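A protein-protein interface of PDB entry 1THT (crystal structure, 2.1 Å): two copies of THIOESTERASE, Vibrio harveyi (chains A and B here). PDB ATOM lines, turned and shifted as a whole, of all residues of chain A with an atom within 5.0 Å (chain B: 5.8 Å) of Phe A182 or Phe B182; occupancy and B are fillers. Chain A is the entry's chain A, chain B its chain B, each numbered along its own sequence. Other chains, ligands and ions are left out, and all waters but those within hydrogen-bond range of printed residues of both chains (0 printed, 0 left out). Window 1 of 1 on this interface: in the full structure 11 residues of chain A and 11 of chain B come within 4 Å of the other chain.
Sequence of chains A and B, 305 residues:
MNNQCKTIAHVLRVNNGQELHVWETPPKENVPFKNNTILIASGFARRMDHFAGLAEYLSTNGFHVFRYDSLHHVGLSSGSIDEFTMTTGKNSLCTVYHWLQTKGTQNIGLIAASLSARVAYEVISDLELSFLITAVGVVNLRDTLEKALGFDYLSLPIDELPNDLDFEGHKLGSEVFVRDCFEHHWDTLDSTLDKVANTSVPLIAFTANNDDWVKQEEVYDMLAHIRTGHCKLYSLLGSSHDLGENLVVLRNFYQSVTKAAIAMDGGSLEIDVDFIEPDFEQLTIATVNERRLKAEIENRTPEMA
NE2 of His A185 lies within hydrogen-bond range of O of Leu B154 (2.8 Å).
The guanidinium group of Arg A179 is in salt-bridge range of the side-chain carboxylate of Glu B183, 2.7 Å away.
A ring nitrogen (NE2) of His B185 lies within hydrogen-bond range of the backbone carbonyl oxygen of Leu A154.
The side-chain carboxylate of Glu A183 is in salt-bridge range of the guanidinium group of Arg B179 (2.8 Å).
Arg B179 touches Arg A179.
CB of Phe B182 touches CB of Phe A182, at 3.9 Å.
OE2 of Glu A183 touches OE2 of Glu B183 (3.5 Å).
Ser B155 touches His A185.
Phe A182 touches one residue of chain B.
Phe B182 touches just one residue of chain A: Phe A182.
Printed residues of chain B within 4 Å of His A185: Leu B154 and Ser B155.
Printed residues of chain B within 4 Å of Arg A179: Arg B179 (3.4 Å) and Glu B183 (2.7 Å).
Printed residues of chain B within 4 Å of Glu A183: Arg B179 and Glu B183.
Of the printed residues of chain A, Glu B183 touches Arg A179 and Glu A183.
Asp A180 touches none of the printed residues of chain B.
Hydrophobic or aromatic side chains of chain B within 4 Å of the printed part of chain A: Phe B182 and His B185.
Hydrophobic or aromatic side chains of chain A that line the printed part of chain B: Phe A182 and His A185.
Leu A154 touches His B185, and with the chains exchanged His A185 touches Leu B154.
Arg A179 touches its own counterpart, Arg B179.
Arg A179 touches Glu B183, and with the chains exchanged Glu A183 touches Arg B179.
Glu A183 touches its own counterpart, Glu B183.
11 positions are printed for both chains.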
ATOM      1  N   ARG A 142      13.274  -3.197   8.297  1.00  0.00           N
ATOM      2  CA  ARG A 142      13.854  -2.705   7.058  1.00  0.00           C
ATOM      3  C   ARG A 142      12.874  -2.770   5.887  1.00  0.00           C
ATOM      4  O   ARG A 142      12.729  -1.767   5.186  1.00  0.00           O
ATOM      5  CB  ARG A 142      15.109  -3.520   6.778  1.00  0.00           C
ATOM      6  CG  ARG A 142      15.808  -3.144   5.490  1.00  0.00           C
ATOM      7  CD  ARG A 142      17.231  -3.617   5.548  1.00  0.00           C
ATOM      8  NE  ARG A 142      17.931  -3.270   4.327  1.00  0.00           N
ATOM      9  CZ  ARG A 142      19.260  -3.115   4.260  1.00  0.00           C
ATOM     10  NH1 ARG A 142      20.043  -3.262   5.332  1.00  0.00           N
ATOM     11  NH2 ARG A 142      19.801  -2.828   3.074  1.00  0.00           N
ATOM     12  N   LEU A 154      18.194   2.228   4.626  1.00  0.00           N
ATOM     13  CA  LEU A 154      19.184   1.489   5.372  1.00  0.00           C
ATOM     14  C   LEU A 154      20.277   0.916   4.460  1.00  0.00           C
ATOM     15  O   LEU A 154      21.268   0.447   4.976  1.00  0.00           O
ATOM     16  CB  LEU A 154      18.469   0.385   6.165  1.00  0.00           C
ATOM     17  CG  LEU A 154      18.142   0.675   7.635  1.00  0.00           C
ATOM     18  CD1 LEU A 154      17.313   1.923   7.808  1.00  0.00           C
ATOM     19  CD2 LEU A 154      17.409  -0.532   8.173  1.00  0.00           C
ATOM     20  N   VAL A 178      18.942   5.283  12.333  1.00  0.00           N
ATOM     21  CA  VAL A 178      19.509   4.197  11.544  1.00  0.00           C
ATOM     22  C   VAL A 178      20.718   3.611  12.284  1.00  0.00           C
ATOM     23  O   VAL A 178      20.852   2.382  12.357  1.00  0.00           O
ATOM     24  CB  VAL A 178      19.910   4.717  10.142  1.00  0.00           C
ATOM     25  CG1 VAL A 178      20.501   3.580   9.349  1.00  0.00           C
ATOM     26  CG2 VAL A 178      18.685   5.158   9.335  1.00  0.00           C
ATOM     27  N   ARG A 179      21.515   4.421  12.987  1.00  0.00           N
ATOM     28  CA  ARG A 179      22.627   3.904  13.750  1.00  0.00           C
ATOM     29  C   ARG A 179      22.093   2.904  14.786  1.00  0.00           C
ATOM     30  O   ARG A 179      22.592   1.766  14.878  1.00  0.00           O
ATOM     31  CB  ARG A 179      23.311   5.033  14.424  1.00  0.00           C
ATOM     32  CG  ARG A 179      24.555   4.572  15.143  1.00  0.00           C
ATOM     33  CD  ARG A 179      25.215   5.684  15.895  1.00  0.00           C
ATOM     34  NE  ARG A 179      25.342   6.813  14.999  1.00  0.00           N
ATOM     35  CZ  ARG A 179      26.454   7.033  14.298  1.00  0.00           C
ATOM     36  NH1 ARG A 179      27.514   6.229  14.391  1.00  0.00           N
ATOM     37  NH2 ARG A 179      26.503   8.063  13.463  1.00  0.00           N
ATOM     38  N   ASP A 180      21.022   3.231  15.520  1.00  0.00           N
ATOM     39  CA  ASP A 180      20.479   2.332  16.523  1.00  0.00           C
ATOM     40  C   ASP A 180      19.929   1.083  15.896  1.00  0.00           C
ATOM     41  O   ASP A 180      20.019   0.031  16.527  1.00  0.00           O
ATOM     42  CB  ASP A 180      19.399   3.065  17.280  1.00  0.00           C
ATOM     43  CG  ASP A 180      18.772   2.257  18.404  1.00  0.00           C
ATOM     44  OD1 ASP A 180      19.446   2.104  19.411  1.00  0.00           O
ATOM     45  OD2 ASP A 180      17.630   1.804  18.288  1.00  0.00           O
ATOM     46  N   CYS A 181      19.317   1.119  14.704  1.00  0.00           N
ATOM     47  CA  CYS A 181      18.827  -0.099  14.062  1.00  0.00           C
ATOM     48  C   CYS A 181      19.899  -1.147  13.947  1.00  0.00           C
ATOM     49  O   CYS A 181      19.630  -2.323  14.195  1.00  0.00           O
ATOM     50  CB  CYS A 181      18.400   0.006  12.630  1.00  0.00           C
ATOM     51  SG  CYS A 181      16.788   0.712  12.356  1.00  0.00           S
ATOM     52  N   PHE A 182      21.092  -0.725  13.509  1.00  0.00           N
ATOM     53  CA  PHE A 182      22.161  -1.663  13.220  1.00  0.00           C
ATOM     54  C   PHE A 182      22.889  -2.155  14.467  1.00  0.00           C
ATOM     55  O   PHE A 182      23.164  -3.339  14.628  1.00  0.00           O
ATOM     56  CB  PHE A 182      23.105  -0.964  12.236  1.00  0.00           C
ATOM     57  CG  PHE A 182      22.581  -0.969  10.806  1.00  0.00           C
ATOM     58  CD1 PHE A 182      22.102  -2.119  10.259  1.00  0.00           C
ATOM     59  CD2 PHE A 182      22.598   0.179  10.048  1.00  0.00           C
ATOM     60  CE1 PHE A 182      21.638  -2.132   8.962  1.00  0.00           C
ATOM     61  CE2 PHE A 182      22.129   0.148   8.749  1.00  0.00           C
ATOM     62  CZ  PHE A 182      21.643  -1.005   8.195  1.00  0.00           C
ATOM     63  N   GLU A 183      23.183  -1.224  15.351  1.00  0.00           N
ATOM     64  CA  GLU A 183      23.805  -1.407  16.625  1.00  0.00           C
ATOM     65  C   GLU A 183      23.009  -2.210  17.634  1.00  0.00           C
ATOM     66  O   GLU A 183      23.584  -2.827  18.544  1.00  0.00           O
ATOM     67  CB  GLU A 183      24.083  -0.060  17.198  1.00  0.00           C
ATOM     68  CG  GLU A 183      25.352   0.285  16.547  1.00  0.00           C
ATOM     69  CD  GLU A 183      25.913   1.657  16.830  1.00  0.00           C
ATOM     70  OE1 GLU A 183      25.777   2.217  17.944  1.00  0.00           O
ATOM     71  OE2 GLU A 183      26.508   2.145  15.861  1.00  0.00           O
ATOM     72  N   HIS A 184      21.673  -2.095  17.606  1.00  0.00           N
ATOM     73  CA  HIS A 184      20.875  -2.916  18.478  1.00  0.00           C
ATOM     74  C   HIS A 184      20.038  -3.939  17.693  1.00  0.00           C
ATOM     75  O   HIS A 184      19.044  -4.475  18.197  1.00  0.00           O
ATOM     76  CB  HIS A 184      20.038  -2.011  19.375  1.00  0.00           C
ATOM     77  CG  HIS A 184      20.907  -1.266  20.384  1.00  0.00           C
ATOM     78  ND1 HIS A 184      21.223  -1.798  21.634  1.00  0.00           N
ATOM     79  CD2 HIS A 184      21.516  -0.061  20.317  1.00  0.00           C
ATOM     80  CE1 HIS A 184      21.991  -0.925  22.265  1.00  0.00           C
ATOM     81  NE2 HIS A 184      22.174   0.117  21.491  1.00  0.00           N
ATOM     82  N   HIS A 185      20.480  -4.185  16.478  1.00  0.00           N
ATOM     83  CA  HIS A 185      19.908  -5.223  15.596  1.00  0.00           C
ATOM     84  C   HIS A 185      18.358  -5.243  15.582  1.00  0.00           C
ATOM     85  O   HIS A 185      17.723  -6.240  15.947  1.00  0.00           O
ATOM     86  CB  HIS A 185      20.373  -6.599  16.097  1.00  0.00           C
ATOM     87  CG  HIS A 185      21.900  -6.730  16.171  1.00  0.00           C
ATOM     88  ND1 HIS A 185      22.631  -6.361  17.301  1.00  0.00           N
ATOM     89  CD2 HIS A 185      22.808  -7.176  15.266  1.00  0.00           C
ATOM     90  CE1 HIS A 185      23.912  -6.587  17.055  1.00  0.00           C
ATOM     91  NE2 HIS A 185      24.033  -7.072  15.845  1.00  0.00           N
ATOM     92  N   ASP A 187      16.728  -4.401  12.755  1.00  0.00           N
ATOM     93  CA  ASP A 187      16.437  -4.306  11.363  1.00  0.00           C
ATOM     94  C   ASP A 187      15.866  -5.439  10.607  1.00  0.00           C
ATOM     95  O   ASP A 187      15.169  -5.144   9.651  1.00  0.00           O
ATOM     96  CB  ASP A 187      17.703  -3.820  10.658  1.00  0.00           C
ATOM     97  CG  ASP A 187      19.022  -4.628  10.867  1.00  0.00           C
ATOM     98  OD1 ASP A 187      19.373  -5.014  11.984  1.00  0.00           O
ATOM     99  OD2 ASP A 187      19.722  -4.847   9.886  1.00  0.00           O
ATOM    100  N   ARG B 142      31.993 -10.559   7.395  1.00  0.00           N
ATOM    101  CA  ARG B 142      31.362 -11.151   8.561  1.00  0.00           C
ATOM    102  C   ARG B 142      31.753 -12.608   8.791  1.00  0.00           C
ATOM    103  O   ARG B 142      32.070 -13.007   9.921  1.00  0.00           O
ATOM    104  CB  ARG B 142      29.841 -10.974   8.400  1.00  0.00           C
ATOM    105  CG  ARG B 142      29.027 -11.553   9.560  1.00  0.00           C
ATOM    106  CD  ARG B 142      27.698 -10.829   9.685  1.00  0.00           C
ATOM    107  NE  ARG B 142      26.996 -11.287  10.865  1.00  0.00           N
ATOM    108  CZ  ARG B 142      26.042 -10.606  11.487  1.00  0.00           C
ATOM    109  NH1 ARG B 142      25.641  -9.394  11.087  1.00  0.00           N
ATOM    110  NH2 ARG B 142      25.454 -11.219  12.511  1.00  0.00           N
ATOM    111  N   LEU B 154      29.504  -9.695  15.305  1.00  0.00           N
ATOM    112  CA  LEU B 154      28.637  -8.700  14.709  1.00  0.00           C
ATOM    113  C   LEU B 154      27.163  -8.940  15.043  1.00  0.00           C
ATOM    114  O   LEU B 154      26.358  -8.086  14.708  1.00  0.00           O
ATOM    115  CB  LEU B 154      28.856  -8.681  13.167  1.00  0.00           C
ATOM    116  CG  LEU B 154      29.862  -7.636  12.616  1.00  0.00           C
ATOM    117  CD1 LEU B 154      31.287  -7.927  13.080  1.00  0.00           C
ATOM    118  CD2 LEU B 154      29.774  -7.651  11.106  1.00  0.00           C
ATOM    119  N   SER B 155      26.816 -10.096  15.621  1.00  0.00           N
ATOM    120  CA  SER B 155      25.472 -10.446  16.050  1.00  0.00           C
ATOM    121  C   SER B 155      25.114  -9.947  17.434  1.00  0.00           C
ATOM    122  O   SER B 155      23.959 -10.090  17.832  1.00  0.00           O
ATOM    123  CB  SER B 155      25.302 -11.940  16.061  1.00  0.00           C
ATOM    124  OG  SER B 155      26.191 -12.555  16.986  1.00  0.00           O
ATOM    125  N   PHE B 177      35.113  -0.355  15.314  1.00  0.00           N
ATOM    126  CA  PHE B 177      35.224  -1.230  14.176  1.00  0.00           C
ATOM    127  C   PHE B 177      33.860  -1.790  13.777  1.00  0.00           C
ATOM    128  O   PHE B 177      33.521  -1.743  12.578  1.00  0.00           O
ATOM    129  CB  PHE B 177      36.194  -2.373  14.505  1.00  0.00           C
ATOM    130  CG  PHE B 177      36.536  -3.240  13.298  1.00  0.00           C
ATOM    131  CD1 PHE B 177      37.521  -2.822  12.409  1.00  0.00           C
ATOM    132  CD2 PHE B 177      35.834  -4.378  13.044  1.00  0.00           C
ATOM    133  CE1 PHE B 177      37.770  -3.572  11.262  1.00  0.00           C
ATOM    134  CE2 PHE B 177      36.101  -5.109  11.897  1.00  0.00           C
ATOM    135  CZ  PHE B 177      37.065  -4.711  11.009  1.00  0.00           C
ATOM    136  N   VAL B 178      33.082  -2.361  14.716  1.00  0.00           N
ATOM    137  CA  VAL B 178      31.781  -2.938  14.364  1.00  0.00           C
ATOM    138  C   VAL B 178      30.789  -1.817  13.919  1.00  0.00           C
ATOM    139  O   VAL B 178      30.108  -1.964  12.896  1.00  0.00           O
ATOM    140  CB  VAL B 178      31.297  -3.761  15.596  1.00  0.00           C
ATOM    141  CG1 VAL B 178      29.945  -4.354  15.342  1.00  0.00           C
ATOM    142  CG2 VAL B 178      32.187  -4.969  15.790  1.00  0.00           C
ATOM    143  N   ARG B 179      30.698  -0.661  14.567  1.00  0.00           N
ATOM    144  CA  ARG B 179      29.887   0.467  14.116  1.00  0.00           C
ATOM    145  C   ARG B 179      30.181   0.783  12.639  1.00  0.00           C
ATOM    146  O   ARG B 179      29.282   0.703  11.784  1.00  0.00           O
ATOM    147  CB  ARG B 179      30.217   1.642  15.022  1.00  0.00           C
ATOM    148  CG  ARG B 179      29.501   2.934  14.686  1.00  0.00           C
ATOM    149  CD  ARG B 179      29.483   3.865  15.862  1.00  0.00           C
ATOM    150  NE  ARG B 179      28.854   3.132  16.952  1.00  0.00           N
ATOM    151  CZ  ARG B 179      29.090   3.345  18.248  1.00  0.00           C
ATOM    152  NH1 ARG B 179      29.949   4.274  18.684  1.00  0.00           N
ATOM    153  NH2 ARG B 179      28.456   2.577  19.132  1.00  0.00           N
ATOM    154  N   ASP B 180      31.445   1.021  12.285  1.00  0.00           N
ATOM    155  CA  ASP B 180      31.826   1.268  10.904  1.00  0.00           C
ATOM    156  C   ASP B 180      31.434   0.184   9.908  1.00  0.00           C
ATOM    157  O   ASP B 180      31.022   0.532   8.798  1.00  0.00           O
ATOM    158  CB  ASP B 180      33.331   1.486  10.839  1.00  0.00           C
ATOM    159  CG  ASP B 180      33.803   1.923   9.455  1.00  0.00           C
ATOM    160  OD1 ASP B 180      33.630   3.091   9.138  1.00  0.00           O
ATOM    161  OD2 ASP B 180      34.315   1.103   8.689  1.00  0.00           O
ATOM    162  N   CYS B 181      31.489  -1.108  10.227  1.00  0.00           N
ATOM    163  CA  CYS B 181      31.114  -2.188   9.293  1.00  0.00           C
ATOM    164  C   CYS B 181      29.689  -2.147   8.804  1.00  0.00           C
ATOM    165  O   CYS B 181      29.367  -2.603   7.699  1.00  0.00           O
ATOM    166  CB  CYS B 181      31.195  -3.617   9.853  1.00  0.00           C
ATOM    167  SG  CYS B 181      32.789  -4.421  10.015  1.00  0.00           S
ATOM    168  N   PHE B 182      28.776  -1.804   9.720  1.00  0.00           N
ATOM    169  CA  PHE B 182      27.354  -1.732   9.361  1.00  0.00           C
ATOM    170  C   PHE B 182      27.031  -0.395   8.668  1.00  0.00           C
ATOM    171  O   PHE B 182      26.334  -0.303   7.673  1.00  0.00           O
ATOM    172  CB  PHE B 182      26.538  -1.874  10.634  1.00  0.00           C
ATOM    173  CG  PHE B 182      26.484  -3.267  11.233  1.00  0.00           C
ATOM    174  CD1 PHE B 182      26.090  -4.344  10.471  1.00  0.00           C
ATOM    175  CD2 PHE B 182      26.793  -3.436  12.570  1.00  0.00           C
ATOM    176  CE1 PHE B 182      25.995  -5.597  11.053  1.00  0.00           C
ATOM    177  CE2 PHE B 182      26.701  -4.690  13.140  1.00  0.00           C
ATOM    178  CZ  PHE B 182      26.300  -5.773  12.384  1.00  0.00           C
ATOM    179  N   GLU B 183      27.513   0.688   9.257  1.00  0.00           N
ATOM    180  CA  GLU B 183      27.359   2.032   8.805  1.00  0.00           C
ATOM    181  C   GLU B 183      27.873   2.350   7.407  1.00  0.00           C
ATOM    182  O   GLU B 183      27.395   3.292   6.766  1.00  0.00           O
ATOM    183  CB  GLU B 183      28.045   2.897   9.805  1.00  0.00           C
ATOM    184  CG  GLU B 183      26.950   3.279  10.752  1.00  0.00           C
ATOM    185  CD  GLU B 183      27.341   4.264  11.841  1.00  0.00           C
ATOM    186  OE1 GLU B 183      28.145   5.182  11.632  1.00  0.00           O
ATOM    187  OE2 GLU B 183      26.794   4.081  12.920  1.00  0.00           O
ATOM    188  N   HIS B 184      28.954   1.663   7.009  1.00  0.00           N
ATOM    189  CA  HIS B 184      29.549   1.820   5.690  1.00  0.00           C
ATOM    190  C   HIS B 184      29.490   0.561   4.845  1.00  0.00           C
ATOM    191  O   HIS B 184      30.116   0.437   3.811  1.00  0.00           O
ATOM    192  CB  HIS B 184      30.977   2.290   5.854  1.00  0.00           C
ATOM    193  CG  HIS B 184      30.985   3.764   6.222  1.00  0.00           C
ATOM    194  ND1 HIS B 184      30.853   4.817   5.414  1.00  0.00           N
ATOM    195  CD2 HIS B 184      31.103   4.234   7.514  1.00  0.00           C
ATOM    196  CE1 HIS B 184      30.883   5.885   6.173  1.00  0.00           C
ATOM    197  NE2 HIS B 184      31.034   5.528   7.436  1.00  0.00           N
ATOM    198  N   HIS B 185      28.640  -0.343   5.246  1.00  0.00           N
ATOM    199  CA  HIS B 185      28.262  -1.597   4.579  1.00  0.00           C
ATOM    200  C   HIS B 185      29.488  -2.389   4.115  1.00  0.00           C
ATOM    201  O   HIS B 185      29.637  -2.711   2.929  1.00  0.00           O
ATOM    202  CB  HIS B 185      27.375  -1.297   3.375  1.00  0.00           C
ATOM    203  CG  HIS B 185      26.093  -0.560   3.755  1.00  0.00           C
ATOM    204  ND1 HIS B 185      26.026   0.829   3.781  1.00  0.00           N
ATOM    205  CD2 HIS B 185      24.864  -1.009   4.116  1.00  0.00           C
ATOM    206  CE1 HIS B 185      24.804   1.173   4.142  1.00  0.00           C
ATOM    207  NE2 HIS B 185      24.098   0.089   4.345  1.00  0.00           N
ATOM    208  N   TRP B 186      30.332  -2.704   5.072  1.00  0.00           N
ATOM    209  CA  TRP B 186      31.556  -3.475   4.826  1.00  0.00           C
ATOM    210  C   TRP B 186      31.326  -4.956   5.101  1.00  0.00           C
ATOM    211  O   TRP B 186      32.124  -5.849   4.803  1.00  0.00           O
ATOM    212  CB  TRP B 186      32.660  -3.031   5.786  1.00  0.00           C
ATOM    213  CG  TRP B 186      33.312  -1.693   5.435  1.00  0.00           C
ATOM    214  CD1 TRP B 186      33.101  -0.517   6.038  1.00  0.00           C
ATOM    215  CD2 TRP B 186      34.262  -1.502   4.406  1.00  0.00           C
ATOM    216  NE1 TRP B 186      33.961   0.431   5.411  1.00  0.00           N
ATOM    217  CE2 TRP B 186      34.645  -0.172   4.466  1.00  0.00           C
ATOM    218  CE3 TRP B 186      34.845  -2.346   3.451  1.00  0.00           C
ATOM    219  CZ2 TRP B 186      35.622   0.369   3.626  1.00  0.00           C
ATOM    220  CZ3 TRP B 186      35.818  -1.788   2.602  1.00  0.00           C
ATOM    221  CH2 TRP B 186      36.191  -0.493   2.690  1.00  0.00           C
ATOM    222  N   ASP B 187      30.194  -5.300   5.681  1.00  0.00           N
ATOM    223  CA  ASP B 187      30.008  -6.632   6.226  1.00  0.00           C
ATOM    224  C   ASP B 187      29.611  -7.821   5.415  1.00  0.00           C
ATOM    225  O   ASP B 187      30.015  -8.931   5.784  1.00  0.00           O
ATOM    226  CB  ASP B 187      29.036  -6.516   7.418  1.00  0.00           C
ATOM    227  CG  ASP B 187      27.638  -5.977   7.116  1.00  0.00           C
ATOM    228  OD1 ASP B 187      27.491  -4.915   6.498  1.00  0.00           O
ATOM    229  OD2 ASP B 187      26.690  -6.622   7.534  1.00  0.00           O
